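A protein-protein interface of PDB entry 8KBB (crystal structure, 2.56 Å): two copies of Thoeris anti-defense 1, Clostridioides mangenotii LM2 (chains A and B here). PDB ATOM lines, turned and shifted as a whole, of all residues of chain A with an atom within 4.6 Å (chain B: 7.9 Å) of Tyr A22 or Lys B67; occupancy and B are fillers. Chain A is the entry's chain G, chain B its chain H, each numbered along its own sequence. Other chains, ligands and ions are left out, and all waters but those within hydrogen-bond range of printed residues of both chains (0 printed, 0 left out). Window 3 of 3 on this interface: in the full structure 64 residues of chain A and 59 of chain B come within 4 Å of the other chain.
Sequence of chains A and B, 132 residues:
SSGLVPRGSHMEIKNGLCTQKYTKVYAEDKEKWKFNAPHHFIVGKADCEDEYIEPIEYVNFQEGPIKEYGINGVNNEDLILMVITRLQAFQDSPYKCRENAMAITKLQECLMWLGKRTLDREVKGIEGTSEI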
ATOM      1  N   GLN A  20      22.586 -21.889 -31.741  1.00  0.00           N
ATOM      2  CA  GLN A  20      21.319 -22.146 -31.036  1.00  0.00           C
ATOM      3  C   GLN A  20      21.093 -23.467 -30.294  1.00  0.00           C
ATOM      4  O   GLN A  20      19.959 -23.804 -30.008  1.00  0.00           O
ATOM      5  CB  GLN A  20      20.091 -21.863 -31.912  1.00  0.00           C
ATOM      6  CG  GLN A  20      19.152 -20.804 -31.363  1.00  0.00           C
ATOM      7  CD  GLN A  20      18.147 -20.332 -32.388  1.00  0.00           C
ATOM      8  OE1 GLN A  20      17.668 -21.110 -33.210  1.00  0.00           O
ATOM      9  NE2 GLN A  20      17.820 -19.053 -32.343  1.00  0.00           N
ATOM     10  N   LYS A  21      22.117 -24.234 -29.988  1.00  0.00           N
ATOM     11  CA  LYS A  21      21.841 -25.484 -29.299  1.00  0.00           C
ATOM     12  C   LYS A  21      21.320 -25.397 -27.886  1.00  0.00           C
ATOM     13  O   LYS A  21      20.447 -26.141 -27.496  1.00  0.00           O
ATOM     14  CB  LYS A  21      23.045 -26.411 -29.322  1.00  0.00           C
ATOM     15  CG  LYS A  21      24.384 -25.750 -29.559  1.00  0.00           C
ATOM     16  CD  LYS A  21      25.528 -26.636 -29.101  1.00  0.00           C
ATOM     17  CE  LYS A  21      26.788 -25.821 -28.856  1.00  0.00           C
ATOM     18  NZ  LYS A  21      27.797 -26.581 -28.063  1.00  0.00           N
ATOM     19  N   TYR A  22      21.879 -24.526 -27.093  1.00  0.00           N
ATOM     20  CA  TYR A  22      21.481 -24.480 -25.714  1.00  0.00           C
ATOM     21  C   TYR A  22      20.892 -23.157 -25.308  1.00  0.00           C
ATOM     22  O   TYR A  22      20.251 -23.056 -24.289  1.00  0.00           O
ATOM     23  CB  TYR A  22      22.699 -24.744 -24.868  1.00  0.00           C
ATOM     24  CG  TYR A  22      23.278 -26.129 -24.927  1.00  0.00           C
ATOM     25  CD1 TYR A  22      22.590 -27.210 -24.410  1.00  0.00           C
ATOM     26  CD2 TYR A  22      24.543 -26.344 -25.441  1.00  0.00           C
ATOM     27  CE1 TYR A  22      23.132 -28.476 -24.436  1.00  0.00           C
ATOM     28  CE2 TYR A  22      25.095 -27.604 -25.472  1.00  0.00           C
ATOM     29  CZ  TYR A  22      24.384 -28.667 -24.968  1.00  0.00           C
ATOM     30  OH  TYR A  22      24.927 -29.929 -24.995  1.00  0.00           O
ATOM     31  N   THR A  23      21.086 -22.133 -26.122  1.00  0.00           N
ATOM     32  CA  THR A  23      20.644 -20.806 -25.764  1.00  0.00           C
ATOM     33  C   THR A  23      19.801 -20.179 -26.828  1.00  0.00           C
ATOM     34  O   THR A  23      19.911 -20.535 -27.982  1.00  0.00           O
ATOM     35  CB  THR A  23      21.852 -19.892 -25.519  1.00  0.00           C
ATOM     36  OG1 THR A  23      22.734 -19.963 -26.638  1.00  0.00           O
ATOM     37  CG2 THR A  23      22.599 -20.287 -24.274  1.00  0.00           C
ATOM     38  N   LYS A  24      18.939 -19.262 -26.445  1.00  0.00           N
ATOM     39  CA  LYS A  24      18.176 -18.519 -27.414  1.00  0.00           C
ATOM     40  C   LYS A  24      18.230 -17.076 -27.058  1.00  0.00           C
ATOM     41  O   LYS A  24      18.335 -16.747 -25.922  1.00  0.00           O
ATOM     42  CB  LYS A  24      16.740 -18.974 -27.484  1.00  0.00           C
ATOM     43  CG  LYS A  24      16.454 -20.115 -28.443  1.00  0.00           C
ATOM     44  CD  LYS A  24      14.985 -20.477 -28.385  1.00  0.00           C
ATOM     45  CE  LYS A  24      14.668 -21.764 -29.114  1.00  0.00           C
ATOM     46  NZ  LYS A  24      14.985 -21.693 -30.560  1.00  0.00           N
ATOM     47  N   GLY A  44      17.738 -17.042 -23.140  1.00  0.00           N
ATOM     48  CA  GLY A  44      16.992 -18.047 -22.420  1.00  0.00           C
ATOM     49  C   GLY A  44      17.417 -19.423 -22.898  1.00  0.00           C
ATOM     50  O   GLY A  44      18.118 -19.566 -23.895  1.00  0.00           O
ATOM     51  N   LYS A  45      16.919 -20.433 -22.217  1.00  0.00           N
ATOM     52  CA  LYS A  45      17.236 -21.769 -22.616  1.00  0.00           C
ATOM     53  C   LYS A  45      16.449 -22.169 -23.807  1.00  0.00           C
ATOM     54  O   LYS A  45      15.277 -21.890 -23.908  1.00  0.00           O
ATOM     55  CB  LYS A  45      17.028 -22.732 -21.489  1.00  0.00           C
ATOM     56  CG  LYS A  45      17.826 -22.450 -20.242  1.00  0.00           C
ATOM     57  CD  LYS A  45      17.829 -23.643 -19.310  1.00  0.00           C
ATOM     58  CE  LYS A  45      18.529 -23.312 -18.008  1.00  0.00           C
ATOM     59  NZ  LYS A  45      18.141 -21.973 -17.503  1.00  0.00           N
ATOM     60  N   ALA A  46      17.123 -22.790 -24.739  1.00  0.00           N
ATOM     61  CA  ALA A  46      16.491 -23.246 -25.933  1.00  0.00           C
ATOM     62  C   ALA A  46      15.455 -24.321 -25.754  1.00  0.00           C
ATOM     63  O   ALA A  46      14.473 -24.341 -26.466  1.00  0.00           O
ATOM     64  CB  ALA A  46      17.533 -23.679 -26.928  1.00  0.00           C
ATOM     65  N   GLN B  62      28.574 -18.890 -19.677  1.00  0.00           N
ATOM     66  CA  GLN B  62      28.541 -20.314 -19.378  1.00  0.00           C
ATOM     67  C   GLN B  62      29.840 -20.729 -18.708  1.00  0.00           C
ATOM     68  O   GLN B  62      30.922 -20.465 -19.226  1.00  0.00           O
ATOM     69  CB  GLN B  62      28.314 -21.120 -20.655  1.00  0.00           C
ATOM     70  CG  GLN B  62      28.172 -22.621 -20.403  1.00  0.00           C
ATOM     71  CD  GLN B  62      27.180 -22.952 -19.288  1.00  0.00           C
ATOM     72  OE1 GLN B  62      26.035 -22.508 -19.295  1.00  0.00           O
ATOM     73  NE2 GLN B  62      27.635 -23.729 -18.311  1.00  0.00           N
ATOM     74  N   GLU B  63      29.732 -21.331 -17.528  1.00  0.00           N
ATOM     75  CA  GLU B  63      30.893 -21.613 -16.686  1.00  0.00           C
ATOM     76  C   GLU B  63      30.922 -23.095 -16.350  1.00  0.00           C
ATOM     77  O   GLU B  63      30.083 -23.580 -15.582  1.00  0.00           O
ATOM     78  CB  GLU B  63      30.865 -20.779 -15.412  1.00  0.00           C
ATOM     79  CG  GLU B  63      32.172 -20.761 -14.688  1.00  0.00           C
ATOM     80  CD  GLU B  63      32.080 -20.012 -13.385  1.00  0.00           C
ATOM     81  OE1 GLU B  63      32.894 -19.090 -13.166  1.00  0.00           O
ATOM     82  OE2 GLU B  63      31.193 -20.349 -12.573  1.00  0.00           O
ATOM     83  N   GLY B  64      31.902 -23.802 -16.893  1.00  0.00           N
ATOM     84  CA  GLY B  64      31.961 -25.232 -16.751  1.00  0.00           C
ATOM     85  C   GLY B  64      31.141 -25.898 -17.831  1.00  0.00           C
ATOM     86  O   GLY B  64      30.383 -25.245 -18.554  1.00  0.00           O
ATOM     87  N   PRO B  65      31.280 -27.216 -17.967  1.00  0.00           N
ATOM     88  CA  PRO B  65      30.491 -27.928 -18.975  1.00  0.00           C
ATOM     89  C   PRO B  65      29.028 -27.911 -18.580  1.00  0.00           C
ATOM     90  O   PRO B  65      28.689 -28.157 -17.416  1.00  0.00           O
ATOM     91  CB  PRO B  65      31.072 -29.344 -18.947  1.00  0.00           C
ATOM     92  CG  PRO B  65      31.584 -29.504 -17.558  1.00  0.00           C
ATOM     93  CD  PRO B  65      31.984 -28.139 -17.057  1.00  0.00           C
ATOM     94  N   ILE B  66      28.163 -27.606 -19.555  1.00  0.00           N
ATOM     95  CA  ILE B  66      26.724 -27.670 -19.314  1.00  0.00           C
ATOM     96  C   ILE B  66      26.368 -29.052 -18.798  1.00  0.00           C
ATOM     97  O   ILE B  66      25.360 -29.239 -18.109  1.00  0.00           O
ATOM     98  CB  ILE B  66      25.945 -27.309 -20.605  1.00  0.00           C
ATOM     99  CG1 ILE B  66      26.240 -25.875 -21.066  1.00  0.00           C
ATOM    100  CG2 ILE B  66      24.452 -27.466 -20.402  1.00  0.00           C
ATOM    101  CD1 ILE B  66      27.411 -25.755 -22.016  1.00  0.00           C
ATOM    102  N   LYS B  67      27.244 -30.020 -19.060  1.00  0.00           N
ATOM    103  CA  LYS B  67      26.991 -31.417 -18.737  1.00  0.00           C
ATOM    104  C   LYS B  67      26.887 -31.667 -17.236  1.00  0.00           C
ATOM    105  O   LYS B  67      26.115 -32.536 -16.812  1.00  0.00           O
ATOM    106  CB  LYS B  67      28.077 -32.295 -19.366  1.00  0.00           C
ATOM    107  CG  LYS B  67      28.091 -32.232 -20.897  1.00  0.00           C
ATOM    108  CD  LYS B  67      26.834 -32.942 -21.457  1.00  0.00           C
ATOM    109  CE  LYS B  67      25.659 -31.993 -21.786  1.00  0.00           C
ATOM    110  NZ  LYS B  67      24.480 -32.731 -22.349  1.00  0.00           N
ATOM    111  N   GLU B  68      27.644 -30.941 -16.402  1.00  0.00           N
ATOM    112  CA  GLU B  68      27.454 -31.142 -14.968  1.00  0.00           C
ATOM    113  C   GLU B  68      26.961 -29.919 -14.205  1.00  0.00           C
ATOM    114  O   GLU B  68      26.376 -30.091 -13.129  1.00  0.00           O
ATOM    115  CB  GLU B  68      28.733 -31.662 -14.280  1.00  0.00           C
ATOM    116  CG  GLU B  68      29.929 -30.728 -14.206  1.00  0.00           C
ATOM    117  CD  GLU B  68      30.910 -31.173 -13.114  1.00  0.00           C
ATOM    118  OE1 GLU B  68      30.576 -32.135 -12.381  1.00  0.00           O
ATOM    119  OE2 GLU B  68      31.993 -30.558 -12.973  1.00  0.00           O
ATOM    120  N   TYR B  69      27.173 -28.707 -14.707  1.00  0.00           N
ATOM    121  CA  TYR B  69      26.617 -27.533 -14.048  1.00  0.00           C
ATOM    122  C   TYR B  69      25.364 -27.010 -14.728  1.00  0.00           C
ATOM    123  O   TYR B  69      24.743 -26.075 -14.214  1.00  0.00           O
ATOM    124  CB  TYR B  69      27.649 -26.405 -13.961  1.00  0.00           C
ATOM    125  CG  TYR B  69      28.931 -26.799 -13.275  1.00  0.00           C
ATOM    126  CD1 TYR B  69      29.060 -26.708 -11.892  1.00  0.00           C
ATOM    127  CD2 TYR B  69      30.028 -27.229 -14.012  1.00  0.00           C
ATOM    128  CE1 TYR B  69      30.238 -27.063 -11.261  1.00  0.00           C
ATOM    129  CE2 TYR B  69      31.209 -27.581 -13.392  1.00  0.00           C
ATOM    130  CZ  TYR B  69      31.311 -27.496 -12.018  1.00  0.00           C
ATOM    131  OH  TYR B  69      32.493 -27.845 -11.404  1.00  0.00           O
ATOM    132  N   GLY B  70      24.976 -27.590 -15.859  1.00  0.00           N
ATOM    133  CA  GLY B  70      23.832 -27.094 -16.588  1.00  0.00           C
ATOM    134  C   GLY B  70      24.136 -25.801 -17.320  1.00  0.00           C
ATOM    135  O   GLY B  70      25.271 -25.317 -17.392  1.00  0.00           O
ATOM    136  N   ILE B  71      23.074 -25.236 -17.882  1.00  0.00           N
ATOM    137  CA  ILE B  71      23.146 -23.955 -18.568  1.00  0.00           C
ATOM    138  C   ILE B  71      23.124 -22.863 -17.503  1.00  0.00           C
ATOM    139  O   ILE B  71      22.137 -22.715 -16.780  1.00  0.00           O
ATOM    140  CB  ILE B  71      21.984 -23.797 -19.549  1.00  0.00           C
ATOM    141  CG1 ILE B  71      22.245 -24.616 -20.807  1.00  0.00           C
ATOM    142  CG2 ILE B  71      21.783 -22.347 -19.888  1.00  0.00           C
ATOM    143  CD1 ILE B  71      21.062 -24.683 -21.698  1.00  0.00           C
ATOM    144  N   GLY B  73      24.878 -19.484 -18.063  1.00  0.00           N
ATOM    145  CA  GLY B  73      25.379 -18.204 -18.530  1.00  0.00           C
ATOM    146  C   GLY B  73      25.245 -18.100 -20.032  1.00  0.00           C
ATOM    147  O   GLY B  73      24.810 -19.039 -20.711  1.00  0.00           O
ATOM    148  N   ASN B  75      26.859 -17.048 -23.997  1.00  0.00           N
ATOM    149  CA  ASN B  75      28.022 -17.316 -24.823  1.00  0.00           C
ATOM    150  C   ASN B  75      28.428 -16.032 -25.525  1.00  0.00           C
ATOM    151  O   ASN B  75      27.591 -15.161 -25.769  1.00  0.00           O
ATOM    152  CB  ASN B  75      27.718 -18.385 -25.860  1.00  0.00           C
ATOM    153  CG  ASN B  75      27.388 -19.710 -25.235  1.00  0.00           C
ATOM    154  OD1 ASN B  75      26.256 -20.183 -25.329  1.00  0.00           O
ATOM    155  ND2 ASN B  75      28.371 -20.322 -24.586  1.00  0.00           N
ATOM    156  N   ASP B  78      26.212 -14.997 -28.263  1.00  0.00           N
ATOM    157  CA  ASP B  78      24.964 -14.317 -27.924  1.00  0.00           C
ATOM    158  C   ASP B  78      25.159 -12.802 -27.857  1.00  0.00           C
ATOM    159  O   ASP B  78      24.345 -12.024 -28.384  1.00  0.00           O
ATOM    160  CB  ASP B  78      24.421 -14.853 -26.595  1.00  0.00           C
ATOM    161  CG  ASP B  78      24.106 -16.349 -26.640  1.00  0.00           C
ATOM    162  OD1 ASP B  78      23.666 -16.851 -27.700  1.00  0.00           O
ATOM    163  OD2 ASP B  78      24.295 -17.024 -25.602  1.00  0.00           O
ATOM    164  N   GLU B 127      33.665 -32.496 -30.308  1.00  0.00           N
ATOM    165  CA  GLU B 127      32.862 -31.309 -30.030  1.00  0.00           C
ATOM    166  C   GLU B 127      32.416 -31.258 -28.573  1.00  0.00           C
ATOM    167  O   GLU B 127      31.902 -32.240 -28.032  1.00  0.00           O
ATOM    168  CB  GLU B 127      31.646 -31.255 -30.960  1.00  0.00           C
ATOM    169  CG  GLU B 127      30.469 -30.452 -30.400  1.00  0.00           C
ATOM    170  CD  GLU B 127      30.694 -28.944 -30.415  1.00  0.00           C
ATOM    171  OE1 GLU B 127      31.843 -28.498 -30.626  1.00  0.00           O
ATOM    172  OE2 GLU B 127      29.712 -28.200 -30.193  1.00  0.00           O
ATOM    173  N   GLY B 128      32.625 -30.102 -27.940  1.00  0.00           N
ATOM    174  CA  GLY B 128      32.180 -29.858 -26.581  1.00  0.00           C
ATOM    175  C   GLY B 128      32.728 -30.820 -25.546  1.00  0.00           C
ATOM    176  O   GLY B 128      31.961 -31.421 -24.788  1.00  0.00           O
ATOM    177  N   THR B 129      34.047 -30.975 -25.497  1.00  0.00           N
ATOM    178  CA  THR B 129      34.675 -31.854 -24.515  1.00  0.00           C
ATOM    179  C   THR B 129      35.255 -31.059 -23.345  1.00  0.00           C
ATOM    180  O   THR B 129      35.150 -29.831 -23.295  1.00  0.00           O
ATOM    181  CB  THR B 129      35.794 -32.707 -25.147  1.00  0.00           C
ATOM    182  OG1 THR B 129      36.610 -31.883 -25.990  1.00  0.00           O
ATOM    183  CG2 THR B 129      35.207 -33.845 -25.972  1.00  0.00           C
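The side-chain hydroxyl (OG1) of Thr A23 is in hydrogen-bond range of the side-chain carboxylate (OD1) of Asp B78.
NZ of Lys A21 is in salt-bridge range of OE2 of Glu B127.
Printed residues of chain B within 4 Å of Lys A45: Ile B71 (3.8 Å).
Lys B67 touches one residue of chain A.
Of the printed residues of chain A, Glu B127 touches Lys A21.
The nearest residue of chain B that does not touch Tyr A22 is Ile B66 (4.4 Å).
Among the printed residues, pairs that only touch across the chains: Tyr A22 with Lys B67, Tyr A22 with Ile B71, Thr A23 with Asn B75 and Lys A45 with Ile B71.
Hydrophobic or aromatic side chains of chain B within 4 Å of the printed part of chain A: Ile B71.
Hydrophobic or aromatic side chains of chain A within 4 Å of the printed part of chain B: Tyr A22.
Among the printed residues, 6 pairs touch across the chains.
Among the printed residues, Asp or Glu carboxylates within 4 Å of a Lys or Arg side-chain nitrogen of the other chain: Lys A21 with Glu B127.
No position is printed for both chains.
Of the 6 pairs that touch across the chains among the printed residues, none has its exchanged pair printed and touching as well.
OD2 of Asp B78 lies within hydrogen-bond range of N of Asn B75.
O of Tyr A22 sits at hydrogen-bond distance from N of Ala A46, 3.2 Å away.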
